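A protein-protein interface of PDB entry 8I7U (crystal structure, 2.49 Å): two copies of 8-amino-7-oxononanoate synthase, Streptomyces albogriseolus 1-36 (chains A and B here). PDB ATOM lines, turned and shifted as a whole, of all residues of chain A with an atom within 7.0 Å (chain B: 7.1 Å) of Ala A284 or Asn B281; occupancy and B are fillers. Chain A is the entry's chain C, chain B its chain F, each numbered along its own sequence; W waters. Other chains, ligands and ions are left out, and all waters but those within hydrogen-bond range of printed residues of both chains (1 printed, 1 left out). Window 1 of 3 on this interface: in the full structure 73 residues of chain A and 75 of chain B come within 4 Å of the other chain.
ND2 of Asn A281 is in hydrogen-bond range of OD1 of Asn B281, 3.3 Å away.
OG of Ser A249 sits at hydrogen-bond distance from ND2 of Asn B281.
The side-chain hydroxyl (OG) of Ser B249 sits at hydrogen-bond distance from the side-chain amide nitrogen (ND2) of Asn A281 (3.2 Å).
The backbone NH (N) of Gly A250 is in hydrogen-bond range of the side-chain amide oxygen (OE1) of Gln B278, 2.8 Å away.
O of Leu A242 sits at hydrogen-bond distance from N of Ala A248.
The backbone carbonyl oxygen of Leu A72 is in hydrogen-bond range of the backbone NH of Thr A282 (2.8 Å).
The side-chain amide nitrogen (ND2) of Asn B105 sits at hydrogen-bond distance from the backbone carbonyl oxygen (O) of Gln B278 (3.0 Å).
The side-chain amide oxygen of Asn B281 is in hydrogen-bond range of the backbone NH of Ala B284.
The backbone carbonyl oxygen (O) of Leu B72 is in hydrogen-bond range of the backbone NH (N) of Thr B282, at 3.0 Å.
OD1 of Asn A281 is in hydrogen-bond range of N of Ala A284 (3.2 Å).
Among the printed residues, pairs that only touch across the chains: Pro A283 with Pro B283 (3.4 Å), Ala A287 with Leu B72 (3.7 Å), Leu A72 with Ala B287 (3.7 Å), Ser A249 with Gln B278 (3.8 Å), Ala A62 with Leu B66 (3.9 Å), Ala A284 with Asn B281 (3.9 Å), Asn A281 with Ala B284 (3.9 Å) and Ala A248 with Leu B72 (3.9 Å).
Printed residues of chain B within 4 Å of Gly A250: Gln B278 (2.8 Å).
Printed residues of chain B within 4 Å of Asn A281: Ser B249 (3.2 Å), Asn B281 (3.3 Å) and Ala B284 (3.9 Å).
Ala A284 touches just one residue of chain B: Asn B281.
Leu B85 touches none of the printed residues of chain A.
Asn B281 touches just these residues of chain A: Ser A249, Asn A281 and Ala A284.
The nearest residue of chain A that does not touch Asn B281 is Pro A283 (4.6 Å).
Printed residues of chain B that touch a printed residue of chain A: Leu B66, Leu B72, Ser B249, Gln B278, Asn B281, Pro B283, Ala B284 and Ala B287.
Hydrophobic or aromatic side chains of chain B within 4 Å of the printed part of chain A: Leu B66, Leu B72, Pro B283, Ala B284 and Ala B287.
Of the 19 printed residues of chain A, 9 touch a printed residue of chain B.
Hydrophobic or aromatic side chains of chain A within 4 Å of the printed part of chain B: Ala A62, Leu A72, Pro A283, Ala A284 and Ala A287.
Among the printed residues, no Asp or Glu carboxylate lies within 4 Å of a Lys or Arg side-chain nitrogen of the other chain.
Leu A72 touches Ala B287, and with the chains exchanged Ala A287 touches Leu B72.
Ser A249 touches Asn B281, and with the chains exchanged Asn A281 touches Ser B249.
Asn A281 touches its own counterpart, Asn B281.
Asn A281 touches Ala B284, and with the chains exchanged Ala A284 touches Asn B281.
Water W1 lies within hydrogen-bond range of OD1 of Asn B73 and OG of Ser A249.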
ATOM      1  N   ALA A  62     -28.461 -15.988  28.548  1.00  0.00           N
ATOM      2  CA  ALA A  62     -27.357 -16.928  28.412  1.00  0.00           C
ATOM      3  C   ALA A  62     -27.825 -18.353  28.680  1.00  0.00           C
ATOM      4  O   ALA A  62     -27.484 -19.277  27.935  1.00  0.00           O
ATOM      5  CB  ALA A  62     -26.210 -16.535  29.351  1.00  0.00           C
ATOM      6  N   ALA A  65     -30.073 -19.498  25.772  1.00  0.00           N
ATOM      7  CA  ALA A  65     -29.358 -19.835  24.543  1.00  0.00           C
ATOM      8  C   ALA A  65     -28.722 -21.215  24.637  1.00  0.00           C
ATOM      9  O   ALA A  65     -28.829 -22.025  23.709  1.00  0.00           O
ATOM     10  CB  ALA A  65     -28.306 -18.780  24.227  1.00  0.00           C
ATOM     11  N   LEU A  72     -22.578 -26.256  23.488  1.00  0.00           N
ATOM     12  CA  LEU A  72     -21.661 -25.212  23.923  1.00  0.00           C
ATOM     13  C   LEU A  72     -21.067 -24.453  22.747  1.00  0.00           C
ATOM     14  O   LEU A  72     -21.259 -23.241  22.642  1.00  0.00           O
ATOM     15  CB  LEU A  72     -20.534 -25.806  24.784  1.00  0.00           C
ATOM     16  CG  LEU A  72     -21.000 -26.184  26.176  1.00  0.00           C
ATOM     17  CD1 LEU A  72     -19.972 -27.062  26.819  1.00  0.00           C
ATOM     18  CD2 LEU A  72     -21.239 -24.905  27.013  1.00  0.00           C
ATOM     19  N   LEU A  85     -27.414 -18.592  16.193  1.00  0.00           N
ATOM     20  CA  LEU A  85     -27.171 -17.775  17.380  1.00  0.00           C
ATOM     21  C   LEU A  85     -25.988 -16.829  17.173  1.00  0.00           C
ATOM     22  O   LEU A  85     -26.064 -15.642  17.512  1.00  0.00           O
ATOM     23  CB  LEU A  85     -26.950 -18.672  18.605  1.00  0.00           C
ATOM     24  CG  LEU A  85     -26.793 -17.942  19.961  1.00  0.00           C
ATOM     25  CD1 LEU A  85     -28.095 -17.302  20.399  1.00  0.00           C
ATOM     26  CD2 LEU A  85     -26.271 -18.849  21.059  1.00  0.00           C
ATOM     27  N   ALA A  89     -26.051 -12.716  17.211  1.00  0.00           N
ATOM     28  CA  ALA A  89     -25.234 -11.926  18.114  1.00  0.00           C
ATOM     29  C   ALA A  89     -24.407 -10.902  17.347  1.00  0.00           C
ATOM     30  O   ALA A  89     -24.297  -9.743  17.761  1.00  0.00           O
ATOM     31  CB  ALA A  89     -24.345 -12.849  18.954  1.00  0.00           C
ATOM     32  N   LEU A 242     -15.942  -7.452  25.790  1.00  0.00           N
ATOM     33  CA  LEU A 242     -17.376  -7.453  26.043  1.00  0.00           C
ATOM     34  C   LEU A 242     -17.733  -7.958  27.435  1.00  0.00           C
ATOM     35  O   LEU A 242     -18.919  -8.168  27.713  1.00  0.00           O
ATOM     36  CB  LEU A 242     -18.107  -8.296  24.999  1.00  0.00           C
ATOM     37  CG  LEU A 242     -17.993  -7.933  23.524  1.00  0.00           C
ATOM     38  CD1 LEU A 242     -18.721  -8.976  22.705  1.00  0.00           C
ATOM     39  CD2 LEU A 242     -18.560  -6.545  23.273  1.00  0.00           C
ATOM     40  N   ALA A 248     -21.174  -9.202  29.134  1.00  0.00           N
ATOM     41  CA  ALA A 248     -21.291 -10.554  28.575  1.00  0.00           C
ATOM     42  C   ALA A 248     -19.948 -11.290  28.582  1.00  0.00           C
ATOM     43  O   ALA A 248     -19.252 -11.288  29.602  1.00  0.00           O
ATOM     44  CB  ALA A 248     -21.873 -10.502  27.153  1.00  0.00           C
ATOM     45  N   SER A 249     -19.567 -11.934  27.470  1.00  0.00           N
ATOM     46  CA  SER A 249     -18.277 -12.625  27.387  1.00  0.00           C
ATOM     47  C   SER A 249     -17.602 -12.330  26.051  1.00  0.00           C
ATOM     48  O   SER A 249     -18.257 -12.031  25.055  1.00  0.00           O
ATOM     49  CB  SER A 249     -18.406 -14.157  27.549  1.00  0.00           C
ATOM     50  OG  SER A 249     -19.120 -14.517  28.724  1.00  0.00           O
ATOM     51  N   GLY A 250     -16.278 -12.428  26.041  1.00  0.00           N
ATOM     52  CA  GLY A 250     -15.525 -12.321  24.810  1.00  0.00           C
ATOM     53  C   GLY A 250     -15.155 -10.903  24.436  1.00  0.00           C
ATOM     54  O   GLY A 250     -15.261  -9.951  25.216  1.00  0.00           O
ATOM     55  N   LEU A 280     -17.059 -17.985  20.369  1.00  0.00           N
ATOM     56  CA  LEU A 280     -17.681 -17.930  21.685  1.00  0.00           C
ATOM     57  C   LEU A 280     -18.693 -19.061  21.848  1.00  0.00           C
ATOM     58  O   LEU A 280     -19.333 -19.487  20.886  1.00  0.00           O
ATOM     59  CB  LEU A 280     -18.380 -16.590  21.894  1.00  0.00           C
ATOM     60  CG  LEU A 280     -17.475 -15.413  22.206  1.00  0.00           C
ATOM     61  CD1 LEU A 280     -18.219 -14.099  22.010  1.00  0.00           C
ATOM     62  CD2 LEU A 280     -16.932 -15.553  23.625  1.00  0.00           C
ATOM     63  N   ASN A 281     -18.850 -19.536  23.087  1.00  0.00           N
ATOM     64  CA  ASN A 281     -19.865 -20.547  23.348  1.00  0.00           C
ATOM     65  C   ASN A 281     -21.253 -19.896  23.405  1.00  0.00           C
ATOM     66  O   ASN A 281     -21.397 -18.670  23.415  1.00  0.00           O
ATOM     67  CB  ASN A 281     -19.554 -21.332  24.626  1.00  0.00           C
ATOM     68  CG  ASN A 281     -19.490 -20.457  25.878  1.00  0.00           C
ATOM     69  OD1 ASN A 281     -20.201 -19.465  25.993  1.00  0.00           O
ATOM     70  ND2 ASN A 281     -18.642 -20.844  26.829  1.00  0.00           N
ATOM     71  N   THR A 282     -22.291 -20.739  23.396  1.00  0.00           N
ATOM     72  CA  THR A 282     -23.644 -20.233  23.183  1.00  0.00           C
ATOM     73  C   THR A 282     -24.157 -19.384  24.338  1.00  0.00           C
ATOM     74  O   THR A 282     -24.861 -18.399  24.081  1.00  0.00           O
ATOM     75  CB  THR A 282     -24.633 -21.374  22.894  1.00  0.00           C
ATOM     76  OG1 THR A 282     -24.477 -22.438  23.842  1.00  0.00           O
ATOM     77  CG2 THR A 282     -24.433 -21.897  21.459  1.00  0.00           C
ATOM     78  N   PRO A 283     -23.868 -19.702  25.609  1.00  0.00           N
ATOM     79  CA  PRO A 283     -24.318 -18.779  26.672  1.00  0.00           C
ATOM     80  C   PRO A 283     -23.756 -17.376  26.503  1.00  0.00           C
ATOM     81  O   PRO A 283     -24.487 -16.385  26.667  1.00  0.00           O
ATOM     82  CB  PRO A 283     -23.835 -19.458  27.965  1.00  0.00           C
ATOM     83  CG  PRO A 283     -22.828 -20.443  27.531  1.00  0.00           C
ATOM     84  CD  PRO A 283     -23.231 -20.900  26.179  1.00  0.00           C
ATOM     85  N   ALA A 284     -22.478 -17.270  26.135  1.00  0.00           N
ATOM     86  CA  ALA A 284     -21.883 -15.961  25.896  1.00  0.00           C
ATOM     87  C   ALA A 284     -22.609 -15.222  24.783  1.00  0.00           C
ATOM     88  O   ALA A 284     -22.824 -14.007  24.874  1.00  0.00           O
ATOM     89  CB  ALA A 284     -20.405 -16.110  25.547  1.00  0.00           C
ATOM     90  N   LEU A 285     -22.978 -15.940  23.714  1.00  0.00           N
ATOM     91  CA  LEU A 285     -23.644 -15.288  22.591  1.00  0.00           C
ATOM     92  C   LEU A 285     -25.070 -14.901  22.964  1.00  0.00           C
ATOM     93  O   LEU A 285     -25.546 -13.820  22.596  1.00  0.00           O
ATOM     94  CB  LEU A 285     -23.618 -16.195  21.357  1.00  0.00           C
ATOM     95  CG  LEU A 285     -22.265 -16.471  20.692  1.00  0.00           C
ATOM     96  CD1 LEU A 285     -22.442 -17.525  19.639  1.00  0.00           C
ATOM     97  CD2 LEU A 285     -21.692 -15.231  20.056  1.00  0.00           C
ATOM     98  N   GLY A 286     -25.757 -15.767  23.707  1.00  0.00           N
ATOM     99  CA  GLY A 286     -27.040 -15.384  24.272  1.00  0.00           C
ATOM    100  C   GLY A 286     -26.952 -14.102  25.077  1.00  0.00           C
ATOM    101  O   GLY A 286     -27.777 -13.198  24.913  1.00  0.00           O
ATOM    102  N   ALA A 287     -25.923 -13.987  25.919  1.00  0.00           N
ATOM    103  CA  ALA A 287     -25.774 -12.792  26.749  1.00  0.00           C
ATOM    104  C   ALA A 287     -25.503 -11.544  25.909  1.00  0.00           C
ATOM    105  O   ALA A 287     -26.027 -10.463  26.216  1.00  0.00           O
ATOM    106  CB  ALA A 287     -24.669 -13.006  27.779  1.00  0.00           C
ATOM    107  N   ILE A 288     -24.699 -11.671  24.845  1.00  0.00           N
ATOM    108  CA  ILE A 288     -24.396 -10.523  23.985  1.00  0.00           C
ATOM    109  C   ILE A 288     -25.658 -10.007  23.296  1.00  0.00           C
ATOM    110  O   ILE A 288     -25.850  -8.795  23.141  1.00  0.00           O
ATOM    111  CB  ILE A 288     -23.313 -10.894  22.956  1.00  0.00           C
ATOM    112  CG1 ILE A 288     -21.927 -10.909  23.599  1.00  0.00           C
ATOM    113  CG2 ILE A 288     -23.344  -9.939  21.766  1.00  0.00           C
ATOM    114  CD1 ILE A 288     -20.935 -11.862  22.927  1.00  0.00           C
ATOM    115  N   ILE A 289     -26.526 -10.915  22.852  1.00  0.00           N
ATOM    116  CA  ILE A 289     -27.764 -10.493  22.205  1.00  0.00           C
ATOM    117  C   ILE A 289     -28.629  -9.703  23.181  1.00  0.00           C
ATOM    118  O   ILE A 289     -29.132  -8.621  22.859  1.00  0.00           O
ATOM    119  CB  ILE A 289     -28.508 -11.717  21.650  1.00  0.00           C
ATOM    120  CG1 ILE A 289     -27.666 -12.339  20.535  1.00  0.00           C
ATOM    121  CG2 ILE A 289     -29.912 -11.327  21.191  1.00  0.00           C
ATOM    122  CD1 ILE A 289     -28.068 -13.725  20.147  1.00  0.00           C
ATOM    123  N   ALA B  65     -23.915 -24.689  36.631  1.00  0.00           N
ATOM    124  CA  ALA B  65     -22.889 -23.771  37.114  1.00  0.00           C
ATOM    125  C   ALA B  65     -23.301 -22.323  36.904  1.00  0.00           C
ATOM    126  O   ALA B  65     -23.020 -21.463  37.743  1.00  0.00           O
ATOM    127  CB  ALA B  65     -21.563 -24.053  36.410  1.00  0.00           C
ATOM    128  N   LEU B  66     -23.973 -22.037  35.785  1.00  0.00           N
ATOM    129  CA  LEU B  66     -24.386 -20.669  35.496  1.00  0.00           C
ATOM    130  C   LEU B  66     -25.533 -20.231  36.389  1.00  0.00           C
ATOM    131  O   LEU B  66     -25.646 -19.045  36.711  1.00  0.00           O
ATOM    132  CB  LEU B  66     -24.781 -20.543  34.028  1.00  0.00           C
ATOM    133  CG  LEU B  66     -25.251 -19.180  33.520  1.00  0.00           C
ATOM    134  CD1 LEU B  66     -24.315 -18.060  33.960  1.00  0.00           C
ATOM    135  CD2 LEU B  66     -25.345 -19.231  31.977  1.00  0.00           C
ATOM    136  N   VAL B  71     -23.465 -15.470  37.713  1.00  0.00           N
ATOM    137  CA  VAL B  71     -22.588 -14.576  36.968  1.00  0.00           C
ATOM    138  C   VAL B  71     -21.955 -15.348  35.823  1.00  0.00           C
ATOM    139  O   VAL B  71     -21.802 -16.570  35.868  1.00  0.00           O
ATOM    140  CB  VAL B  71     -21.472 -13.927  37.822  1.00  0.00           C
ATOM    141  CG1 VAL B  71     -22.052 -12.867  38.710  1.00  0.00           C
ATOM    142  CG2 VAL B  71     -20.703 -14.983  38.633  1.00  0.00           C
ATOM    143  N   LEU B  72     -21.575 -14.599  34.795  1.00  0.00           N
ATOM    144  CA  LEU B  72     -20.746 -15.111  33.720  1.00  0.00           C
ATOM    145  C   LEU B  72     -19.269 -15.145  34.112  1.00  0.00           C
ATOM    146  O   LEU B  72     -18.628 -16.201  34.052  1.00  0.00           O
ATOM    147  CB  LEU B  72     -20.954 -14.256  32.476  1.00  0.00           C
ATOM    148  CG  LEU B  72     -22.259 -14.592  31.781  1.00  0.00           C
ATOM    149  CD1 LEU B  72     -22.599 -13.532  30.758  1.00  0.00           C
ATOM    150  CD2 LEU B  72     -22.093 -15.965  31.147  1.00  0.00           C
ATOM    151  N   ASN B  73     -18.704 -13.996  34.503  1.00  0.00           N
ATOM    152  CA  ASN B  73     -17.277 -13.924  34.790  1.00  0.00           C
ATOM    153  C   ASN B  73     -16.903 -14.869  35.918  1.00  0.00           C
ATOM    154  O   ASN B  73     -17.638 -15.019  36.889  1.00  0.00           O
ATOM    155  CB  ASN B  73     -16.866 -12.503  35.161  1.00  0.00           C
ATOM    156  CG  ASN B  73     -16.757 -11.609  33.968  1.00  0.00           C
ATOM    157  OD1 ASN B  73     -16.773 -12.069  32.819  1.00  0.00           O
ATOM    158  ND2 ASN B  73     -16.624 -10.310  34.225  1.00  0.00           N
ATOM    159  N   SER B  74     -15.774 -15.556  35.754  1.00  0.00           N
ATOM    160  CA  SER B  74     -15.212 -16.383  36.818  1.00  0.00           C
ATOM    161  C   SER B  74     -14.187 -15.623  37.640  1.00  0.00           C
ATOM    162  O   SER B  74     -13.645 -16.159  38.612  1.00  0.00           O
ATOM    163  CB  SER B  74     -14.594 -17.639  36.226  1.00  0.00           C
ATOM    164  OG  SER B  74     -13.369 -17.334  35.594  1.00  0.00           O
ATOM    165  N   LEU B  83     -13.581 -17.146  41.425  1.00  0.00           N
ATOM    166  CA  LEU B  83     -14.689 -17.942  41.951  1.00  0.00           C
ATOM    167  C   LEU B  83     -14.224 -19.346  42.356  1.00  0.00           C
ATOM    168  O   LEU B  83     -13.316 -19.917  41.740  1.00  0.00           O
ATOM    169  CB  LEU B  83     -15.801 -18.082  40.911  1.00  0.00           C
ATOM    170  CG  LEU B  83     -16.603 -16.874  40.429  1.00  0.00           C
ATOM    171  CD1 LEU B  83     -17.661 -17.322  39.430  1.00  0.00           C
ATOM    172  CD2 LEU B  83     -17.248 -16.178  41.597  1.00  0.00           C
ATOM    173  N   LEU B  85     -15.708 -21.943  41.595  1.00  0.00           N
ATOM    174  CA  LEU B  85     -15.894 -22.770  40.407  1.00  0.00           C
ATOM    175  C   LEU B  85     -14.601 -22.892  39.604  1.00  0.00           C
ATOM    176  O   LEU B  85     -14.225 -23.990  39.183  1.00  0.00           O
ATOM    177  CB  LEU B  85     -17.017 -22.197  39.546  1.00  0.00           C
ATOM    178  CG  LEU B  85     -17.477 -23.014  38.335  1.00  0.00           C
ATOM    179  CD1 LEU B  85     -18.121 -24.323  38.771  1.00  0.00           C
ATOM    180  CD2 LEU B  85     -18.457 -22.189  37.514  1.00  0.00           C
ATOM    181  N   ASN B 105      -9.090 -18.835  28.049  1.00  0.00           N
ATOM    182  CA  ASN B 105     -10.244 -18.789  27.172  1.00  0.00           C
ATOM    183  C   ASN B 105     -10.000 -19.518  25.855  1.00  0.00           C
ATOM    184  O   ASN B 105     -10.954 -19.746  25.103  1.00  0.00           O
ATOM    185  CB  ASN B 105     -10.643 -17.335  26.930  1.00  0.00           C
ATOM    186  CG  ASN B 105      -9.509 -16.517  26.357  1.00  0.00           C
ATOM    187  OD1 ASN B 105      -8.839 -16.938  25.396  1.00  0.00           O
ATOM    188  ND2 ASN B 105      -9.270 -15.345  26.939  1.00  0.00           N
ATOM    189  N   SER B 249     -15.028 -26.012  26.842  1.00  0.00           N
ATOM    190  CA  SER B 249     -14.829 -24.699  26.281  1.00  0.00           C
ATOM    191  C   SER B 249     -13.478 -24.219  26.804  1.00  0.00           C
ATOM    192  O   SER B 249     -12.998 -24.733  27.818  1.00  0.00           O
ATOM    193  CB  SER B 249     -16.055 -23.859  26.662  1.00  0.00           C
ATOM    194  OG  SER B 249     -16.156 -22.653  25.961  1.00  0.00           O
ATOM    195  N   GLN B 278      -9.441 -12.193  29.817  1.00  0.00           N
ATOM    196  CA  GLN B 278     -10.570 -12.690  30.593  1.00  0.00           C
ATOM    197  C   GLN B 278     -10.526 -14.207  30.751  1.00  0.00           C
ATOM    198  O   GLN B 278     -10.159 -14.947  29.825  1.00  0.00           O
ATOM    199  CB  GLN B 278     -11.885 -12.267  29.914  1.00  0.00           C
ATOM    200  CG  GLN B 278     -12.110 -12.852  28.484  1.00  0.00           C
ATOM    201  CD  GLN B 278     -13.389 -12.345  27.867  1.00  0.00           C
ATOM    202  OE1 GLN B 278     -14.448 -12.918  28.079  1.00  0.00           O
ATOM    203  NE2 GLN B 278     -13.305 -11.245  27.132  1.00  0.00           N
ATOM    204  N   ARG B 279     -10.911 -14.666  31.938  1.00  0.00           N
ATOM    205  CA  ARG B 279     -10.961 -16.090  32.212  1.00  0.00           C
ATOM    206  C   ARG B 279     -12.249 -16.686  31.643  1.00  0.00           C
ATOM    207  O   ARG B 279     -13.159 -15.966  31.231  1.00  0.00           O
ATOM    208  CB  ARG B 279     -10.864 -16.338  33.719  1.00  0.00           C
ATOM    209  CG  ARG B 279      -9.882 -15.400  34.429  1.00  0.00           C
ATOM    210  CD  ARG B 279      -8.938 -16.171  35.320  1.00  0.00           C
ATOM    211  NE  ARG B 279      -7.781 -15.383  35.742  1.00  0.00           N
ATOM    212  CZ  ARG B 279      -6.772 -15.867  36.459  1.00  0.00           C
ATOM    213  NH1 ARG B 279      -6.718 -17.146  36.807  1.00  0.00           N
ATOM    214  NH2 ARG B 279      -5.791 -15.051  36.835  1.00  0.00           N
ATOM    215  N   LEU B 280     -12.313 -18.018  31.602  1.00  0.00           N
ATOM    216  CA  LEU B 280     -13.496 -18.702  31.094  1.00  0.00           C
ATOM    217  C   LEU B 280     -14.727 -18.322  31.918  1.00  0.00           C
ATOM    218  O   LEU B 280     -14.640 -18.089  33.125  1.00  0.00           O
ATOM    219  CB  LEU B 280     -13.290 -20.225  31.133  1.00  0.00           C
ATOM    220  CG  LEU B 280     -12.393 -20.782  30.027  1.00  0.00           C
ATOM    221  CD1 LEU B 280     -12.022 -22.257  30.276  1.00  0.00           C
ATOM    222  CD2 LEU B 280     -13.065 -20.571  28.665  1.00  0.00           C
ATOM    223  N   ASN B 281     -15.885 -18.252  31.248  1.00  0.00           N
ATOM    224  CA  ASN B 281     -17.150 -17.992  31.918  1.00  0.00           C
ATOM    225  C   ASN B 281     -17.621 -19.247  32.658  1.00  0.00           C
ATOM    226  O   ASN B 281     -17.023 -20.319  32.565  1.00  0.00           O
ATOM    227  CB  ASN B 281     -18.217 -17.472  30.932  1.00  0.00           C
ATOM    228  CG  ASN B 281     -18.539 -18.463  29.778  1.00  0.00           C
ATOM    229  OD1 ASN B 281     -18.264 -19.661  29.859  1.00  0.00           O
ATOM    230  ND2 ASN B 281     -19.125 -17.944  28.712  1.00  0.00           N
ATOM    231  N   THR B 282     -18.704 -19.098  33.428  1.00  0.00           N
ATOM    232  CA  THR B 282     -19.078 -20.128  34.386  1.00  0.00           C
ATOM    233  C   THR B 282     -19.689 -21.363  33.729  1.00  0.00           C
ATOM    234  O   THR B 282     -19.487 -22.469  34.249  1.00  0.00           O
ATOM    235  CB  THR B 282     -20.036 -19.574  35.449  1.00  0.00           C
ATOM    236  OG1 THR B 282     -21.077 -18.802  34.826  1.00  0.00           O
ATOM    237  CG2 THR B 282     -19.264 -18.713  36.439  1.00  0.00           C
ATOM    238  N   PRO B 283     -20.451 -21.249  32.625  1.00  0.00           N
ATOM    239  CA  PRO B 283     -20.914 -22.488  31.967  1.00  0.00           C
ATOM    240  C   PRO B 283     -19.773 -23.329  31.431  1.00  0.00           C
ATOM    241  O   PRO B 283     -19.798 -24.550  31.595  1.00  0.00           O
ATOM    242  CB  PRO B 283     -21.848 -21.982  30.852  1.00  0.00           C
ATOM    243  CG  PRO B 283     -21.568 -20.542  30.727  1.00  0.00           C
ATOM    244  CD  PRO B 283     -21.143 -20.074  32.069  1.00  0.00           C
ATOM    245  N   ALA B 284     -18.751 -22.705  30.839  1.00  0.00           N
ATOM    246  CA  ALA B 284     -17.582 -23.454  30.384  1.00  0.00           C
ATOM    247  C   ALA B 284     -16.888 -24.164  31.541  1.00  0.00           C
ATOM    248  O   ALA B 284     -16.515 -25.337  31.428  1.00  0.00           O
ATOM    249  CB  ALA B 284     -16.601 -22.520  29.670  1.00  0.00           C
ATOM    250  N   LEU B 285     -16.686 -23.467  32.655  1.00  0.00           N
ATOM    251  CA  LEU B 285     -15.993 -24.090  33.776  1.00  0.00           C
ATOM    252  C   LEU B 285     -16.810 -25.242  34.344  1.00  0.00           C
ATOM    253  O   LEU B 285     -16.262 -26.308  34.649  1.00  0.00           O
ATOM    254  CB  LEU B 285     -15.682 -23.052  34.856  1.00  0.00           C
ATOM    255  CG  LEU B 285     -14.657 -21.966  34.510  1.00  0.00           C
ATOM    256  CD1 LEU B 285     -14.609 -20.951  35.596  1.00  0.00           C
ATOM    257  CD2 LEU B 285     -13.288 -22.556  34.330  1.00  0.00           C
ATOM    258  N   GLY B 286     -18.125 -25.056  34.462  1.00  0.00           N
ATOM    259  CA  GLY B 286     -18.985 -26.158  34.864  1.00  0.00           C
ATOM    260  C   GLY B 286     -18.853 -27.357  33.947  1.00  0.00           C
ATOM    261  O   GLY B 286     -18.762 -28.502  34.406  1.00  0.00           O
ATOM    262  N   ALA B 287     -18.823 -27.102  32.633  1.00  0.00           N
ATOM    263  CA  ALA B 287     -18.623 -28.159  31.648  1.00  0.00           C
ATOM    264  C   ALA B 287     -17.292 -28.867  31.868  1.00  0.00           C
ATOM    265  O   ALA B 287     -17.224 -30.103  31.878  1.00  0.00           O
ATOM    266  CB  ALA B 287     -18.693 -27.572  30.235  1.00  0.00           C
HETATM  267  O   HOH W   1     -16.807 -14.198  30.725  1.00  0.00           O
